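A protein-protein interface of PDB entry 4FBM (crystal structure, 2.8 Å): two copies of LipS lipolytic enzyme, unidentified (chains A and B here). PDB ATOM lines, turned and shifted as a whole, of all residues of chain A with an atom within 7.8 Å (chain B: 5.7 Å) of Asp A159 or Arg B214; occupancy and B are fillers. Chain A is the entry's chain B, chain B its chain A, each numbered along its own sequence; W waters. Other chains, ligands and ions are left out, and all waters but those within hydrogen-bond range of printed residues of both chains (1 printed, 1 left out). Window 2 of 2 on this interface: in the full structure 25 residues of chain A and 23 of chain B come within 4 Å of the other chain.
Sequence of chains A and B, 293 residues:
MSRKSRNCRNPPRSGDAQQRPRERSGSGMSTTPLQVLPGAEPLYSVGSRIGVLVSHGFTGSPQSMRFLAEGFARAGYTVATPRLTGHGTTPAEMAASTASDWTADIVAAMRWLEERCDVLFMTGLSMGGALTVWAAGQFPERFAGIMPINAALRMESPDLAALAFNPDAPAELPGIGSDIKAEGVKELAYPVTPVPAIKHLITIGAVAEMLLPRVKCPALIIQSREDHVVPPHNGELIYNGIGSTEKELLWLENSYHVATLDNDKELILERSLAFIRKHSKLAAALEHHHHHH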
ATOM      1  N   GLU A 156     -14.632 -14.681  27.110  1.00  0.00           N
ATOM      2  CA  GLU A 156     -16.099 -14.700  27.136  1.00  0.00           C
ATOM      3  C   GLU A 156     -16.784 -13.422  26.598  1.00  0.00           C
ATOM      4  O   GLU A 156     -17.674 -12.870  27.226  1.00  0.00           O
ATOM      5  CB  GLU A 156     -16.636 -15.137  28.506  1.00  0.00           C
ATOM      6  CG  GLU A 156     -17.342 -16.495  28.433  1.00  0.00           C
ATOM      7  CD  GLU A 156     -17.202 -17.378  29.686  1.00  0.00           C
ATOM      8  OE1 GLU A 156     -16.525 -16.995  30.656  1.00  0.00           O
ATOM      9  OE2 GLU A 156     -17.773 -18.486  29.703  1.00  0.00           O
ATOM     10  N   SER A 157     -16.359 -12.971  25.423  1.00  0.00           N
ATOM     11  CA  SER A 157     -16.887 -11.752  24.830  1.00  0.00           C
ATOM     12  C   SER A 157     -17.202 -11.887  23.319  1.00  0.00           C
ATOM     13  O   SER A 157     -16.306 -11.937  22.497  1.00  0.00           O
ATOM     14  CB  SER A 157     -15.910 -10.600  25.083  1.00  0.00           C
ATOM     15  OG  SER A 157     -15.445 -10.067  23.871  1.00  0.00           O
ATOM     16  N   PRO A 158     -18.482 -11.901  22.945  1.00  0.00           N
ATOM     17  CA  PRO A 158     -18.741 -12.176  21.544  1.00  0.00           C
ATOM     18  C   PRO A 158     -18.293 -11.068  20.639  1.00  0.00           C
ATOM     19  O   PRO A 158     -18.044 -11.311  19.477  1.00  0.00           O
ATOM     20  CB  PRO A 158     -20.260 -12.367  21.497  1.00  0.00           C
ATOM     21  CG  PRO A 158     -20.628 -12.713  22.866  1.00  0.00           C
ATOM     22  CD  PRO A 158     -19.732 -11.881  23.716  1.00  0.00           C
ATOM     23  N   ASP A 159     -18.226  -9.863  21.160  1.00  0.00           N
ATOM     24  CA  ASP A 159     -17.830  -8.716  20.382  1.00  0.00           C
ATOM     25  C   ASP A 159     -16.381  -8.796  19.993  1.00  0.00           C
ATOM     26  O   ASP A 159     -15.976  -8.201  19.011  1.00  0.00           O
ATOM     27  CB  ASP A 159     -18.089  -7.443  21.166  1.00  0.00           C
ATOM     28  CG  ASP A 159     -19.512  -6.962  21.019  1.00  0.00           C
ATOM     29  OD1 ASP A 159     -19.886  -6.549  19.900  1.00  0.00           O
ATOM     30  OD2 ASP A 159     -20.264  -7.000  22.014  1.00  0.00           O
ATOM     31  N   LEU A 160     -15.599  -9.530  20.778  1.00  0.00           N
ATOM     32  CA  LEU A 160     -14.167  -9.637  20.550  1.00  0.00           C
ATOM     33  C   LEU A 160     -13.935 -10.693  19.507  1.00  0.00           C
ATOM     34  O   LEU A 160     -13.093 -10.542  18.638  1.00  0.00           O
ATOM     35  CB  LEU A 160     -13.447 -10.002  21.844  1.00  0.00           C
ATOM     36  CG  LEU A 160     -11.925  -9.824  21.996  1.00  0.00           C
ATOM     37  CD1 LEU A 160     -11.418  -8.362  22.038  1.00  0.00           C
ATOM     38  CD2 LEU A 160     -11.534 -10.521  23.256  1.00  0.00           C
ATOM     39  N   ALA A 161     -14.693 -11.772  19.608  1.00  0.00           N
ATOM     40  CA  ALA A 161     -14.635 -12.847  18.645  1.00  0.00           C
ATOM     41  C   ALA A 161     -15.089 -12.387  17.266  1.00  0.00           C
ATOM     42  O   ALA A 161     -14.608 -12.874  16.250  1.00  0.00           O
ATOM     43  CB  ALA A 161     -15.476 -13.981  19.113  1.00  0.00           C
ATOM     44  N   ALA A 162     -16.009 -11.434  17.217  1.00  0.00           N
ATOM     45  CA  ALA A 162     -16.443 -10.910  15.924  1.00  0.00           C
ATOM     46  C   ALA A 162     -15.317 -10.153  15.191  1.00  0.00           C
ATOM     47  O   ALA A 162     -15.389  -9.964  13.979  1.00  0.00           O
ATOM     48  CB  ALA A 162     -17.688 -10.054  16.083  1.00  0.00           C
ATOM     49  N   LEU A 163     -14.264  -9.771  15.906  1.00  0.00           N
ATOM     50  CA  LEU A 163     -13.134  -9.088  15.281  1.00  0.00           C
ATOM     51  C   LEU A 163     -11.970 -10.007  14.853  1.00  0.00           C
ATOM     52  O   LEU A 163     -11.104  -9.613  14.071  1.00  0.00           O
ATOM     53  CB  LEU A 163     -12.634  -8.001  16.208  1.00  0.00           C
ATOM     54  CG  LEU A 163     -13.623  -6.895  16.550  1.00  0.00           C
ATOM     55  CD1 LEU A 163     -13.249  -6.224  17.838  1.00  0.00           C
ATOM     56  CD2 LEU A 163     -13.646  -5.910  15.421  1.00  0.00           C
ATOM     57  N   ALA A 164     -11.960 -11.238  15.346  1.00  0.00           N
ATOM     58  CA  ALA A 164     -10.889 -12.170  15.056  1.00  0.00           C
ATOM     59  C   ALA A 164     -10.660 -12.423  13.564  1.00  0.00           C
ATOM     60  O   ALA A 164      -9.522 -12.408  13.111  1.00  0.00           O
ATOM     61  CB  ALA A 164     -11.152 -13.457  15.776  1.00  0.00           C
ATOM     62  N   ASN A 166     -12.782 -10.882  10.947  1.00  0.00           N
ATOM     63  CA  ASN A 166     -13.707  -9.994  10.273  1.00  0.00           C
ATOM     64  C   ASN A 166     -12.960  -9.245   9.181  1.00  0.00           C
ATOM     65  O   ASN A 166     -12.064  -8.455   9.479  1.00  0.00           O
ATOM     66  CB  ASN A 166     -14.364  -9.066  11.294  1.00  0.00           C
ATOM     67  CG  ASN A 166     -15.251  -8.007  10.665  1.00  0.00           C
ATOM     68  OD1 ASN A 166     -15.219  -7.776   9.453  1.00  0.00           O
ATOM     69  ND2 ASN A 166     -16.038  -7.333  11.502  1.00  0.00           N
ATOM     70  N   LEU A 173      -8.626  -0.403  17.338  1.00  0.00           N
ATOM     71  CA  LEU A 173      -9.759  -0.171  18.248  1.00  0.00           C
ATOM     72  C   LEU A 173      -9.316   0.423  19.577  1.00  0.00           C
ATOM     73  O   LEU A 173      -8.120   0.433  19.866  1.00  0.00           O
ATOM     74  CB  LEU A 173     -10.550  -1.460  18.494  1.00  0.00           C
ATOM     75  CG  LEU A 173     -11.628  -1.836  17.463  1.00  0.00           C
ATOM     76  CD1 LEU A 173     -12.685  -2.692  18.171  1.00  0.00           C
ATOM     77  CD2 LEU A 173     -12.288  -0.611  16.721  1.00  0.00           C
ATOM     78  N   ILE A 198      -5.937 -10.011  17.677  1.00  0.00           N
ATOM     79  CA  ILE A 198      -6.945 -10.484  18.594  1.00  0.00           C
ATOM     80  C   ILE A 198      -7.033 -12.022  18.544  1.00  0.00           C
ATOM     81  O   ILE A 198      -7.117 -12.683  19.590  1.00  0.00           O
ATOM     82  CB  ILE A 198      -8.316  -9.894  18.255  1.00  0.00           C
ATOM     83  CG1 ILE A 198      -8.298  -8.345  18.368  1.00  0.00           C
ATOM     84  CG2 ILE A 198      -9.403 -10.623  19.074  1.00  0.00           C
ATOM     85  CD1 ILE A 198      -9.669  -7.597  18.418  1.00  0.00           C
ATOM     86  N   ALA B 136     -22.380 -17.856  11.179  1.00  0.00           N
ATOM     87  CA  ALA B 136     -23.683 -17.400  11.578  1.00  0.00           C
ATOM     88  C   ALA B 136     -23.477 -16.290  12.557  1.00  0.00           C
ATOM     89  O   ALA B 136     -24.254 -15.332  12.575  1.00  0.00           O
ATOM     90  CB  ALA B 136     -24.485 -18.502  12.181  1.00  0.00           C
ATOM     91  N   GLY B 137     -22.411 -16.379  13.344  1.00  0.00           N
ATOM     92  CA  GLY B 137     -22.179 -15.381  14.374  1.00  0.00           C
ATOM     93  C   GLY B 137     -21.463 -14.176  13.820  1.00  0.00           C
ATOM     94  O   GLY B 137     -21.630 -13.082  14.328  1.00  0.00           O
ATOM     95  N   GLN B 138     -20.640 -14.380  12.792  1.00  0.00           N
ATOM     96  CA  GLN B 138     -19.904 -13.269  12.198  1.00  0.00           C
ATOM     97  C   GLN B 138     -20.837 -12.411  11.364  1.00  0.00           C
ATOM     98  O   GLN B 138     -20.707 -11.189  11.338  1.00  0.00           O
ATOM     99  CB  GLN B 138     -18.728 -13.736  11.335  1.00  0.00           C
ATOM    100  CG  GLN B 138     -17.930 -12.583  10.716  1.00  0.00           C
ATOM    101  CD  GLN B 138     -17.001 -11.941  11.700  1.00  0.00           C
ATOM    102  OE1 GLN B 138     -15.866 -12.351  11.869  1.00  0.00           O
ATOM    103  NE2 GLN B 138     -17.469 -10.930  12.350  1.00  0.00           N
ATOM    104  N   PHE B 139     -21.774 -13.060  10.690  1.00  0.00           N
ATOM    105  CA  PHE B 139     -22.726 -12.375   9.849  1.00  0.00           C
ATOM    106  C   PHE B 139     -24.161 -12.637  10.327  1.00  0.00           C
ATOM    107  O   PHE B 139     -24.948 -13.304   9.660  1.00  0.00           O
ATOM    108  CB  PHE B 139     -22.503 -12.831   8.426  1.00  0.00           C
ATOM    109  CG  PHE B 139     -21.075 -12.740   8.004  1.00  0.00           C
ATOM    110  CD1 PHE B 139     -20.305 -13.890   7.833  1.00  0.00           C
ATOM    111  CD2 PHE B 139     -20.473 -11.488   7.789  1.00  0.00           C
ATOM    112  CE1 PHE B 139     -18.960 -13.805   7.432  1.00  0.00           C
ATOM    113  CE2 PHE B 139     -19.130 -11.392   7.399  1.00  0.00           C
ATOM    114  CZ  PHE B 139     -18.373 -12.554   7.223  1.00  0.00           C
ATOM    115  N   PRO B 140     -24.500 -12.100  11.496  1.00  0.00           N
ATOM    116  CA  PRO B 140     -25.749 -12.356  12.190  1.00  0.00           C
ATOM    117  C   PRO B 140     -27.001 -12.369  11.296  1.00  0.00           C
ATOM    118  O   PRO B 140     -27.844 -13.272  11.432  1.00  0.00           O
ATOM    119  CB  PRO B 140     -25.834 -11.182  13.162  1.00  0.00           C
ATOM    120  CG  PRO B 140     -24.435 -10.769  13.413  1.00  0.00           C
ATOM    121  CD  PRO B 140     -23.728 -11.010  12.119  1.00  0.00           C
ATOM    122  N   LEU B 211     -18.625 -16.925  19.854  1.00  0.00           N
ATOM    123  CA  LEU B 211     -19.695 -16.319  19.052  1.00  0.00           C
ATOM    124  C   LEU B 211     -21.104 -16.901  19.228  1.00  0.00           C
ATOM    125  O   LEU B 211     -22.034 -16.342  18.686  1.00  0.00           O
ATOM    126  CB  LEU B 211     -19.340 -16.357  17.564  1.00  0.00           C
ATOM    127  CG  LEU B 211     -18.239 -15.456  17.001  1.00  0.00           C
ATOM    128  CD1 LEU B 211     -17.949 -15.818  15.571  1.00  0.00           C
ATOM    129  CD2 LEU B 211     -18.570 -13.982  17.095  1.00  0.00           C
ATOM    130  N   LEU B 212     -21.289 -18.001  19.969  1.00  0.00           N
ATOM    131  CA  LEU B 212     -22.628 -18.628  20.093  1.00  0.00           C
ATOM    132  C   LEU B 212     -23.723 -17.648  20.525  1.00  0.00           C
ATOM    133  O   LEU B 212     -24.812 -17.648  19.941  1.00  0.00           O
ATOM    134  CB  LEU B 212     -22.620 -19.851  21.003  1.00  0.00           C
ATOM    135  CG  LEU B 212     -21.958 -21.114  20.438  1.00  0.00           C
ATOM    136  CD1 LEU B 212     -21.946 -22.283  21.447  1.00  0.00           C
ATOM    137  CD2 LEU B 212     -22.599 -21.559  19.127  1.00  0.00           C
ATOM    138  N   PRO B 213     -23.435 -16.780  21.514  1.00  0.00           N
ATOM    139  CA  PRO B 213     -24.488 -15.846  21.878  1.00  0.00           C
ATOM    140  C   PRO B 213     -25.072 -15.048  20.699  1.00  0.00           C
ATOM    141  O   PRO B 213     -26.248 -14.671  20.769  1.00  0.00           O
ATOM    142  CB  PRO B 213     -23.805 -14.908  22.887  1.00  0.00           C
ATOM    143  CG  PRO B 213     -22.783 -15.738  23.520  1.00  0.00           C
ATOM    144  CD  PRO B 213     -22.274 -16.664  22.413  1.00  0.00           C
ATOM    145  N   ARG B 214     -24.292 -14.804  19.638  1.00  0.00           N
ATOM    146  CA  ARG B 214     -24.751 -13.932  18.530  1.00  0.00           C
ATOM    147  C   ARG B 214     -25.418 -14.637  17.347  1.00  0.00           C
ATOM    148  O   ARG B 214     -25.963 -13.978  16.443  1.00  0.00           O
ATOM    149  CB  ARG B 214     -23.608 -13.108  17.984  1.00  0.00           C
ATOM    150  CG  ARG B 214     -23.266 -11.948  18.808  1.00  0.00           C
ATOM    151  CD  ARG B 214     -21.891 -11.504  18.420  1.00  0.00           C
ATOM    152  NE  ARG B 214     -21.728 -11.229  16.989  1.00  0.00           N
ATOM    153  CZ  ARG B 214     -21.298 -10.069  16.479  1.00  0.00           C
ATOM    154  NH1 ARG B 214     -20.987  -9.048  17.285  1.00  0.00           N
ATOM    155  NH2 ARG B 214     -21.177  -9.933  15.154  1.00  0.00           N
ATOM    156  N   VAL B 215     -25.336 -15.961  17.316  1.00  0.00           N
ATOM    157  CA  VAL B 215     -26.091 -16.728  16.353  1.00  0.00           C
ATOM    158  C   VAL B 215     -27.535 -16.629  16.813  1.00  0.00           C
ATOM    159  O   VAL B 215     -27.840 -17.035  17.937  1.00  0.00           O
ATOM    160  CB  VAL B 215     -25.650 -18.180  16.384  1.00  0.00           C
ATOM    161  CG1 VAL B 215     -26.619 -19.047  15.635  1.00  0.00           C
ATOM    162  CG2 VAL B 215     -24.219 -18.297  15.825  1.00  0.00           C
ATOM    163  N   LYS B 216     -28.424 -16.061  15.994  1.00  0.00           N
ATOM    164  CA  LYS B 216     -29.842 -15.986  16.395  1.00  0.00           C
ATOM    165  C   LYS B 216     -30.800 -16.705  15.423  1.00  0.00           C
ATOM    166  O   LYS B 216     -32.008 -16.827  15.673  1.00  0.00           O
ATOM    167  CB  LYS B 216     -30.254 -14.548  16.672  1.00  0.00           C
ATOM    168  CG  LYS B 216     -30.015 -13.619  15.509  1.00  0.00           C
ATOM    169  CD  LYS B 216     -31.226 -13.544  14.559  1.00  0.00           C
ATOM    170  CE  LYS B 216     -31.023 -12.473  13.479  1.00  0.00           C
ATOM    171  NZ  LYS B 216     -30.148 -11.331  13.923  1.00  0.00           N
ATOM    172  N   GLY B 243     -28.105 -17.844  21.074  1.00  0.00           N
ATOM    173  CA  GLY B 243     -29.237 -16.936  21.317  1.00  0.00           C
ATOM    174  C   GLY B 243     -30.391 -17.211  20.360  1.00  0.00           C
ATOM    175  O   GLY B 243     -31.490 -16.646  20.487  1.00  0.00           O
HETATM  176  O   HOH W   1     -14.293 -13.488  13.486  1.00  0.00           O
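The side-chain amide nitrogen of Gln B138 sits at hydrogen-bond distance from the backbone carbonyl oxygen of Ala A162 (2.8 Å). The guanidinium group (NH1) of Arg B214 is in salt-bridge range of the side-chain carboxylate (OD1) of Asp A159 (3.8 Å).
Of the printed residues of chain B, Pro A158 touches Leu B211, Pro B213 and Arg B214. Asp A159 touches one residue of chain B. Of the printed residues of chain B, Ala A162 touches Gln B138 (2.8 Å), Leu B211 (3.6 Å) and Arg B214 (3.6 Å). Ala B136 touches none of the printed residues of chain A. Gly B137 touches none of the printed residues of chain A. Of the printed residues of chain A, Leu B211 touches Pro A158 (3.6 Å), Ala A161 (3.7 Å) and Ala A162 (3.6 Å). Arg B214 touches three residues of chain A. The nearest residue of chain A that does not touch Arg B214 is Leu A160 (6.4 Å). The nearest printed residue of chain B that does not touch Pro A158 is Leu B212 (5.9 Å).
Leu B211 touches Pro A158. Pro A158 touches Pro B213 (CG to CG, 3.8 Å). Arg B214 touches Pro A158 (CD to CB, 3.6 Å). Ala A161 touches Leu B211 (CB to CD2, 3.7 Å). Leu B211 touches Ala A162. Ala A162 touches Arg B214. Asn A166 touches Gln B138.
Water W1 lies within hydrogen-bond range of OE1 of Gln B138 (2.5 Å) and O of Ala A161 (2.8 Å).
Of the 12 printed residues of chain A, 5 touch a printed residue of chain B. Printed residues of chain A that touch a printed residue of chain B: Pro A158, Asp A159, Ala A161, Ala A162 and Asn A166. Hydrophobic or aromatic side chains of chain A within 4 Å of the printed part of chain B: Pro A158, Ala A161 and Ala A162. Of the 12 printed residues of chain B, 4 touch a printed residue of chain A. Printed residues of chain B that touch a printed residue of chain A: Gln B138, Leu B211, Pro B213 and Arg B214. Hydrophobic or aromatic side chains of chain B that line the printed part of chain A: Leu B211 and Pro B213. Among the printed residues, 9 pairs touch across the chains.
No position is printed for both chains. Of the 9 pairs that touch across the chains among the printed residues, none has its exchanged pair printed and touching as well.
The backbone carbonyl oxygen (O) of Gly B137 lies within hydrogen-bond range of the guanidinium group (NE) of Arg B214 (3.2 Å).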
